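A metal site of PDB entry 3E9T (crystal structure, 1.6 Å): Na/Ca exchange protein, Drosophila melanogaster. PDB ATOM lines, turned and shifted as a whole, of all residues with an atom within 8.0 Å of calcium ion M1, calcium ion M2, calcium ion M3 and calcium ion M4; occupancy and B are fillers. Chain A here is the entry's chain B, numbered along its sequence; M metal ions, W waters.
The backbone NH (N) of Ile 75 is in hydrogen-bond range of the backbone carbonyl oxygen (O) of Asp 51 (2.9 Å).
N of Glu 16 lies within hydrogen-bond range of O of Leu 110 (2.8 Å).
N of Ser 47 lies close to OD1 of Asp 51, 2.8 Å away.
O of Glu 84 is in hydrogen-bond range of N of Ile 109.
The side-chain hydroxyl of Thr 50 lies close to the side-chain carboxylate of Asp 51 (3.1 Å).
The side-chain amide nitrogen (ND2) of Asn 17 sits at hydrogen-bond distance from the side-chain carboxylate (OD2) of Asp 112 (3.4 Å).
Water W5 bridges the backbone carbonyl oxygen of Thr 45 (3.1 Å) and the side-chain carboxylate of Glu 84 (3.3 Å).
Water W6 bridges O of Ile 75 (2.8 Å) and O of Asp 51 (2.8 Å).
Water W2 bridges OD1 of Asp 77 (2.7 Å) and O of Thr 50 (3.1 Å).
Six residues have an atom within 4 Å of calcium ion M2: Glu 16, Asp 77, Val 79, Glu 81, Asp 111 and Asp 113.
The nearest printed residue that does not touch calcium ion M2 is Phe 80 (4.3 Å).
Three residues have an atom within 4 Å of calcium ion M3: Glu 16, Asp 51 and Glu 81.
Calcium ion M3 is bound by water W2 (2.3 Å), OE1 of Glu 16 (2.4 Å), OE2 of Glu 81 (2.5 Å), OD2 of Asp 51 (2.6 Å), water W1 (2.7 Å), water W6 (2.7 Å), OE1 of Glu 81 (2.7 Å) and water W3 (2.8 Å).
Calcium ion M2 is bound by OD2 of Asp 113, O of Val 79, OD2 of Asp 77, OD1 of Asp 111, OE2 of Glu 16, OE1 of Glu 81 and OE1 of Glu 16.
Three residues have an atom within 4 Å of calcium ion M1: Asp 51, Glu 81 and Glu 84.
The nearest printed residue that does not touch calcium ion M1 is Thr 50 (4.5 Å).
The nearest printed residue that does not touch calcium ion M4 is Asp 78 (4.4 Å).
Calcium ion M1 is bound by water W5, water W4, the side-chain carboxylate (OD2) of Asp 51, the side-chain carboxylate (OE2) of Glu 81, the side-chain carboxylate (OE1) of Glu 84 and the side-chain carboxylate (OD1) of Asp 51.
Calcium ion M1 has six donor atoms within binding distance.
OD2 of Asp 76 binds calcium ion M4, 2.2 Å away.
Calcium ion M4 is bound by O of Asp 77 (2.2 Å).
OD1 of Asp 113 binds calcium ion M4, at 2.4 Å.
The side-chain carboxylate (OD1) of Asp 112 is bound to calcium ion M4.
OE2 of Glu 16 is bound to calcium ion M4, at 2.6 Å.
OD2 of Asp 113 binds calcium ion M4 (2.8 Å).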
ATOM      1  N   MET A  15      30.764 -26.691   7.276  1.00  0.00           N
ATOM      2  CA  MET A  15      29.704 -26.725   6.304  1.00  0.00           C
ATOM      3  C   MET A  15      28.501 -25.948   6.831  1.00  0.00           C
ATOM      4  O   MET A  15      28.223 -25.981   8.041  1.00  0.00           O
ATOM      5  CB  MET A  15      29.289 -28.179   6.040  1.00  0.00           C
ATOM      6  CG  MET A  15      30.381 -29.077   5.481  1.00  0.00           C
ATOM      7  SD  MET A  15      31.305 -28.361   4.116  1.00  0.00           S
ATOM      8  CE  MET A  15      30.121 -28.370   2.787  1.00  0.00           C
ATOM      9  N   GLU A  16      27.772 -25.301   5.937  1.00  0.00           N
ATOM     10  CA  GLU A  16      26.586 -24.535   6.327  1.00  0.00           C
ATOM     11  C   GLU A  16      25.550 -25.379   7.065  1.00  0.00           C
ATOM     12  O   GLU A  16      24.824 -24.856   7.896  1.00  0.00           O
ATOM     13  CB  GLU A  16      25.944 -23.878   5.115  1.00  0.00           C
ATOM     14  CG  GLU A  16      24.844 -22.928   5.540  1.00  0.00           C
ATOM     15  CD  GLU A  16      24.122 -22.311   4.369  1.00  0.00           C
ATOM     16  OE1 GLU A  16      24.005 -21.067   4.346  1.00  0.00           O
ATOM     17  OE2 GLU A  16      23.669 -23.059   3.491  1.00  0.00           O
ATOM     18  N   ASN A  17      25.487 -26.677   6.759  1.00  0.00           N
ATOM     19  CA  ASN A  17      24.527 -27.574   7.405  1.00  0.00           C
ATOM     20  C   ASN A  17      25.072 -28.355   8.611  1.00  0.00           C
ATOM     21  O   ASN A  17      24.501 -29.378   8.996  1.00  0.00           O
ATOM     22  CB  ASN A  17      23.916 -28.531   6.376  1.00  0.00           C
ATOM     23  CG  ASN A  17      24.950 -29.435   5.721  1.00  0.00           C
ATOM     24  OD1 ASN A  17      26.163 -29.188   5.819  1.00  0.00           O
ATOM     25  ND2 ASN A  17      24.485 -30.483   5.070  1.00  0.00           N
ATOM     26  N   CYS A  18      26.160 -27.860   9.224  1.00  0.00           N
ATOM     27  CA  CYS A  18      26.795 -28.545  10.354  1.00  0.00           C
ATOM     28  C   CYS A  18      25.975 -28.455  11.655  1.00  0.00           C
ATOM     29  O   CYS A  18      26.194 -29.241  12.586  1.00  0.00           O
ATOM     30  CB  CYS A  18      28.207 -27.996  10.603  1.00  0.00           C
ATOM     31  SG  CYS A  18      28.283 -26.364  11.336  1.00  0.00           S
ATOM     32  N   THR A  45      32.538 -11.537   5.854  1.00  0.00           N
ATOM     33  CA  THR A  45      31.584 -11.649   4.742  1.00  0.00           C
ATOM     34  C   THR A  45      30.362 -12.476   5.147  1.00  0.00           C
ATOM     35  O   THR A  45      29.297 -12.351   4.534  1.00  0.00           O
ATOM     36  CB  THR A  45      32.239 -12.216   3.464  1.00  0.00           C
ATOM     37  OG1 THR A  45      33.020 -13.370   3.790  1.00  0.00           O
ATOM     38  CG2 THR A  45      33.137 -11.159   2.836  1.00  0.00           C
ATOM     39  N   ALA A  46      30.518 -13.317   6.174  1.00  0.00           N
ATOM     40  CA  ALA A  46      29.381 -13.988   6.814  1.00  0.00           C
ATOM     41  C   ALA A  46      28.871 -13.131   7.984  1.00  0.00           C
ATOM     42  O   ALA A  46      29.666 -12.490   8.689  1.00  0.00           O
ATOM     43  CB  ALA A  46      29.791 -15.363   7.301  1.00  0.00           C
ATOM     44  N   SER A  47      27.559 -13.127   8.192  1.00  0.00           N
ATOM     45  CA  SER A  47      26.938 -12.171   9.116  1.00  0.00           C
ATOM     46  C   SER A  47      26.085 -12.825  10.188  1.00  0.00           C
ATOM     47  O   SER A  47      25.331 -13.752   9.887  1.00  0.00           O
ATOM     48  CB  SER A  47      26.071 -11.196   8.328  1.00  0.00           C
ATOM     49  OG  SER A  47      26.842 -10.534   7.349  1.00  0.00           O
ATOM     50  N   THR A  50      22.244 -14.131   9.807  1.00  0.00           N
ATOM     51  CA  THR A  50      21.971 -14.709   8.497  1.00  0.00           C
ATOM     52  C   THR A  50      22.783 -16.000   8.270  1.00  0.00           C
ATOM     53  O   THR A  50      22.250 -16.986   7.777  1.00  0.00           O
ATOM     54  CB  THR A  50      22.164 -13.700   7.318  1.00  0.00           C
ATOM     55  OG1 THR A  50      23.536 -13.388   7.163  1.00  0.00           O
ATOM     56  CG2 THR A  50      21.432 -12.396   7.565  1.00  0.00           C
ATOM     57  N   ASP A  51      24.053 -15.993   8.674  1.00  0.00           N
ATOM     58  CA  ASP A  51      24.968 -17.120   8.440  1.00  0.00           C
ATOM     59  C   ASP A  51      25.346 -17.899   9.685  1.00  0.00           C
ATOM     60  O   ASP A  51      25.694 -19.083   9.618  1.00  0.00           O
ATOM     61  CB  ASP A  51      26.246 -16.630   7.754  1.00  0.00           C
ATOM     62  CG  ASP A  51      25.959 -15.958   6.446  1.00  0.00           C
ATOM     63  OD1 ASP A  51      26.184 -14.739   6.347  1.00  0.00           O
ATOM     64  OD2 ASP A  51      25.457 -16.661   5.545  1.00  0.00           O
ATOM     65  N   PHE A  52      25.300 -17.230  10.831  1.00  0.00           N
ATOM     66  CA  PHE A  52      25.611 -17.893  12.093  1.00  0.00           C
ATOM     67  C   PHE A  52      24.874 -17.134  13.171  1.00  0.00           C
ATOM     68  O   PHE A  52      24.447 -16.022  12.944  1.00  0.00           O
ATOM     69  CB  PHE A  52      27.117 -17.900  12.381  1.00  0.00           C
ATOM     70  CG  PHE A  52      27.742 -16.501  12.510  1.00  0.00           C
ATOM     71  CD1 PHE A  52      28.206 -15.813  11.376  1.00  0.00           C
ATOM     72  CD2 PHE A  52      27.866 -15.892  13.745  1.00  0.00           C
ATOM     73  CE1 PHE A  52      28.767 -14.526  11.477  1.00  0.00           C
ATOM     74  CE2 PHE A  52      28.437 -14.606  13.856  1.00  0.00           C
ATOM     75  CZ  PHE A  52      28.902 -13.946  12.717  1.00  0.00           C
ATOM     76  N   VAL A  74      25.541 -22.496  13.369  1.00  0.00           N
ATOM     77  CA  VAL A  74      25.633 -22.062  11.976  1.00  0.00           C
ATOM     78  C   VAL A  74      24.221 -22.159  11.367  1.00  0.00           C
ATOM     79  O   VAL A  74      23.477 -23.124  11.634  1.00  0.00           O
ATOM     80  CB  VAL A  74      26.670 -22.924  11.208  1.00  0.00           C
ATOM     81  CG1 VAL A  74      26.705 -22.547   9.722  1.00  0.00           C
ATOM     82  CG2 VAL A  74      28.086 -22.742  11.824  1.00  0.00           C
ATOM     83  N   ILE A  75      23.840 -21.112  10.631  1.00  0.00           N
ATOM     84  CA  ILE A  75      22.485 -21.019  10.060  1.00  0.00           C
ATOM     85  C   ILE A  75      22.439 -21.632   8.662  1.00  0.00           C
ATOM     86  O   ILE A  75      23.163 -21.229   7.763  1.00  0.00           O
ATOM     87  CB  ILE A  75      21.920 -19.559  10.068  1.00  0.00           C
ATOM     88  CG1 ILE A  75      21.851 -19.023  11.509  1.00  0.00           C
ATOM     89  CG2 ILE A  75      20.528 -19.510   9.372  1.00  0.00           C
ATOM     90  CD1 ILE A  75      21.436 -17.554  11.616  1.00  0.00           C
ATOM     91  N   ASP A  76      21.569 -22.632   8.501  1.00  0.00           N
ATOM     92  CA  ASP A  76      21.421 -23.299   7.231  1.00  0.00           C
ATOM     93  C   ASP A  76      20.300 -22.636   6.447  1.00  0.00           C
ATOM     94  O   ASP A  76      19.277 -22.276   7.011  1.00  0.00           O
ATOM     95  CB  ASP A  76      21.090 -24.788   7.452  1.00  0.00           C
ATOM     96  CG  ASP A  76      21.296 -25.636   6.208  1.00  0.00           C
ATOM     97  OD1 ASP A  76      20.865 -26.803   6.225  1.00  0.00           O
ATOM     98  OD2 ASP A  76      21.895 -25.151   5.225  1.00  0.00           O
ATOM     99  N   ASP A  77      20.500 -22.461   5.153  1.00  0.00           N
ATOM    100  CA  ASP A  77      19.371 -22.105   4.282  1.00  0.00           C
ATOM    101  C   ASP A  77      19.385 -22.906   2.982  1.00  0.00           C
ATOM    102  O   ASP A  77      20.159 -23.859   2.834  1.00  0.00           O
ATOM    103  CB  ASP A  77      19.253 -20.587   4.054  1.00  0.00           C
ATOM    104  CG  ASP A  77      20.501 -19.971   3.463  1.00  0.00           C
ATOM    105  OD1 ASP A  77      20.814 -18.818   3.831  1.00  0.00           O
ATOM    106  OD2 ASP A  77      21.165 -20.618   2.631  1.00  0.00           O
ATOM    107  N   ASP A  78      18.495 -22.546   2.057  1.00  0.00           N
ATOM    108  CA  ASP A  78      18.387 -23.249   0.790  1.00  0.00           C
ATOM    109  C   ASP A  78      18.972 -22.408  -0.338  1.00  0.00           C
ATOM    110  O   ASP A  78      18.861 -22.759  -1.520  1.00  0.00           O
ATOM    111  CB  ASP A  78      16.904 -23.561   0.484  1.00  0.00           C
ATOM    112  CG  ASP A  78      16.328 -24.656   1.387  1.00  0.00           C
ATOM    113  OD1 ASP A  78      17.024 -25.119   2.332  1.00  0.00           O
ATOM    114  OD2 ASP A  78      15.164 -25.063   1.149  1.00  0.00           O
ATOM    115  N   VAL A  79      19.598 -21.289   0.037  1.00  0.00           N
ATOM    116  CA  VAL A  79      20.172 -20.351  -0.916  1.00  0.00           C
ATOM    117  C   VAL A  79      21.656 -20.665  -1.127  1.00  0.00           C
ATOM    118  O   VAL A  79      22.435 -20.737  -0.175  1.00  0.00           O
ATOM    119  CB  VAL A  79      20.027 -18.887  -0.409  1.00  0.00           C
ATOM    120  CG1 VAL A  79      20.551 -17.900  -1.438  1.00  0.00           C
ATOM    121  CG2 VAL A  79      18.557 -18.573  -0.075  1.00  0.00           C
ATOM    122  N   PHE A  80      22.037 -20.847  -2.397  1.00  0.00           N
ATOM    123  CA  PHE A  80      23.445 -20.993  -2.754  1.00  0.00           C
ATOM    124  C   PHE A  80      24.226 -19.734  -2.372  1.00  0.00           C
ATOM    125  O   PHE A  80      23.766 -18.614  -2.615  1.00  0.00           O
ATOM    126  CB  PHE A  80      23.589 -21.256  -4.261  1.00  0.00           C
ATOM    127  CG  PHE A  80      24.905 -20.815  -4.825  1.00  0.00           C
ATOM    128  CD1 PHE A  80      25.004 -19.626  -5.543  1.00  0.00           C
ATOM    129  CD2 PHE A  80      26.062 -21.563  -4.604  1.00  0.00           C
ATOM    130  CE1 PHE A  80      26.232 -19.197  -6.054  1.00  0.00           C
ATOM    131  CE2 PHE A  80      27.295 -21.142  -5.112  1.00  0.00           C
ATOM    132  CZ  PHE A  80      27.372 -19.959  -5.838  1.00  0.00           C
ATOM    133  N   GLU A  81      25.385 -19.944  -1.746  1.00  0.00           N
ATOM    134  CA  GLU A  81      26.327 -18.848  -1.429  1.00  0.00           C
ATOM    135  C   GLU A  81      27.780 -19.252  -1.702  1.00  0.00           C
ATOM    136  O   GLU A  81      28.119 -20.429  -1.652  1.00  0.00           O
ATOM    137  CB  GLU A  81      26.227 -18.426   0.041  1.00  0.00           C
ATOM    138  CG  GLU A  81      24.845 -17.971   0.487  1.00  0.00           C
ATOM    139  CD  GLU A  81      24.637 -18.234   1.948  1.00  0.00           C
ATOM    140  OE1 GLU A  81      23.961 -19.237   2.282  1.00  0.00           O
ATOM    141  OE2 GLU A  81      25.182 -17.466   2.779  1.00  0.00           O
ATOM    142  N   GLU A  82      28.631 -18.266  -1.948  1.00  0.00           N
ATOM    143  CA  GLU A  82      30.057 -18.490  -2.069  1.00  0.00           C
ATOM    144  C   GLU A  82      30.666 -18.748  -0.679  1.00  0.00           C
ATOM    145  O   GLU A  82      29.974 -18.566   0.332  1.00  0.00           O
ATOM    146  CB  GLU A  82      30.691 -17.276  -2.742  1.00  0.00           C
ATOM    147  CG  GLU A  82      29.965 -16.921  -4.054  1.00  0.00           C
ATOM    148  CD  GLU A  82      30.615 -15.801  -4.842  1.00  0.00           C
ATOM    149  OE1 GLU A  82      30.121 -15.503  -5.951  1.00  0.00           O
ATOM    150  OE2 GLU A  82      31.607 -15.199  -4.363  1.00  0.00           O
ATOM    151  N   ASP A  83      31.926 -19.178  -0.613  1.00  0.00           N
ATOM    152  CA  ASP A  83      32.574 -19.355   0.692  1.00  0.00           C
ATOM    153  C   ASP A  83      32.603 -18.001   1.405  1.00  0.00           C
ATOM    154  O   ASP A  83      32.958 -16.996   0.802  1.00  0.00           O
ATOM    155  CB  ASP A  83      34.014 -19.853   0.580  1.00  0.00           C
ATOM    156  CG  ASP A  83      34.110 -21.229  -0.063  1.00  0.00           C
ATOM    157  OD1 ASP A  83      33.051 -21.850  -0.332  1.00  0.00           O
ATOM    158  OD2 ASP A  83      35.254 -21.696  -0.331  1.00  0.00           O
ATOM    159  N   GLU A  84      32.240 -17.985   2.685  1.00  0.00           N
ATOM    160  CA  GLU A  84      32.223 -16.730   3.458  1.00  0.00           C
ATOM    161  C   GLU A  84      32.871 -16.938   4.812  1.00  0.00           C
ATOM    162  O   GLU A  84      32.854 -18.039   5.334  1.00  0.00           O
ATOM    163  CB  GLU A  84      30.809 -16.208   3.640  1.00  0.00           C
ATOM    164  CG  GLU A  84      30.136 -15.843   2.325  1.00  0.00           C
ATOM    165  CD  GLU A  84      28.741 -15.273   2.493  1.00  0.00           C
ATOM    166  OE1 GLU A  84      28.062 -15.599   3.492  1.00  0.00           O
ATOM    167  OE2 GLU A  84      28.326 -14.508   1.597  1.00  0.00           O
ATOM    168  N   ILE A 109      32.753 -20.674   6.254  1.00  0.00           N
ATOM    169  CA  ILE A 109      31.551 -21.450   6.068  1.00  0.00           C
ATOM    170  C   ILE A 109      31.484 -21.826   4.590  1.00  0.00           C
ATOM    171  O   ILE A 109      31.537 -20.954   3.708  1.00  0.00           O
ATOM    172  CB  ILE A 109      30.256 -20.664   6.444  1.00  0.00           C
ATOM    173  CG1 ILE A 109      30.250 -20.207   7.898  1.00  0.00           C
ATOM    174  CG2 ILE A 109      28.994 -21.545   6.152  1.00  0.00           C
ATOM    175  CD1 ILE A 109      29.147 -19.170   8.201  1.00  0.00           C
ATOM    176  N   LEU A 110      31.373 -23.122   4.338  1.00  0.00           N
ATOM    177  CA  LEU A 110      31.205 -23.646   2.983  1.00  0.00           C
ATOM    178  C   LEU A 110      29.747 -23.993   2.761  1.00  0.00           C
ATOM    179  O   LEU A 110      29.137 -24.640   3.605  1.00  0.00           O
ATOM    180  CB  LEU A 110      32.054 -24.901   2.772  1.00  0.00           C
ATOM    181  CG  LEU A 110      33.523 -24.815   3.210  1.00  0.00           C
ATOM    182  CD1 LEU A 110      34.203 -26.135   2.924  1.00  0.00           C
ATOM    183  CD2 LEU A 110      34.247 -23.637   2.516  1.00  0.00           C
ATOM    184  N   ASP A 111      29.194 -23.545   1.643  1.00  0.00           N
ATOM    185  CA  ASP A 111      27.781 -23.745   1.329  1.00  0.00           C
ATOM    186  C   ASP A 111      27.535 -25.180   0.867  1.00  0.00           C
ATOM    187  O   ASP A 111      28.437 -25.827   0.323  1.00  0.00           O
ATOM    188  CB  ASP A 111      27.344 -22.747   0.255  1.00  0.00           C
ATOM    189  CG  ASP A 111      25.843 -22.499   0.230  1.00  0.00           C
ATOM    190  OD1 ASP A 111      25.332 -21.743   1.089  1.00  0.00           O
ATOM    191  OD2 ASP A 111      25.177 -23.020  -0.675  1.00  0.00           O
ATOM    192  N   ASP A 112      26.312 -25.667   1.067  1.00  0.00           N
ATOM    193  CA  ASP A 112      25.918 -27.024   0.664  1.00  0.00           C
ATOM    194  C   ASP A 112      24.798 -27.045  -0.388  1.00  0.00           C
ATOM    195  O   ASP A 112      24.384 -28.113  -0.845  1.00  0.00           O
ATOM    196  CB  ASP A 112      25.488 -27.837   1.900  1.00  0.00           C
ATOM    197  CG  ASP A 112      24.266 -27.234   2.594  1.00  0.00           C
ATOM    198  OD1 ASP A 112      24.187 -25.991   2.742  1.00  0.00           O
ATOM    199  OD2 ASP A 112      23.363 -28.000   3.003  1.00  0.00           O
ATOM    200  N   ASP A 113      24.327 -25.855  -0.778  1.00  0.00           N
ATOM    201  CA  ASP A 113      23.147 -25.704  -1.643  1.00  0.00           C
ATOM    202  C   ASP A 113      23.478 -25.696  -3.140  1.00  0.00           C
ATOM    203  O   ASP A 113      24.034 -24.725  -3.675  1.00  0.00           O
ATOM    204  CB  ASP A 113      22.368 -24.435  -1.254  1.00  0.00           C
ATOM    205  CG  ASP A 113      22.076 -24.376   0.239  1.00  0.00           C
ATOM    206  OD1 ASP A 113      21.562 -25.395   0.774  1.00  0.00           O
ATOM    207  OD2 ASP A 113      22.345 -23.340   0.885  1.00  0.00           O
HETATM  208 CA    CA M   1      25.556 -15.132   3.577  1.00  0.00          CA
HETATM  209 CA    CA M   2      23.091 -21.555   1.732  1.00  0.00          CA
HETATM  210 CA    CA M   3      25.279 -19.091   4.632  1.00  0.00          CA
HETATM  211 CA    CA M   4      22.018 -25.044   3.061  1.00  0.00          CA
HETATM  212  O   HOH W   1      27.827 -18.325   4.654  1.00  0.00           O
HETATM  213  O   HOH W   2      23.096 -18.490   5.195  1.00  0.00           O
HETATM  214  O   HOH W   3      26.757 -20.924   3.074  1.00  0.00           O
HETATM  215  O   HOH W   4      24.576 -14.436   1.565  1.00  0.00           O
HETATM  216  O   HOH W   5      26.359 -13.277   3.966  1.00  0.00           O
HETATM  217  O   HOH W   6      25.611 -20.165   7.067  1.00  0.00           O
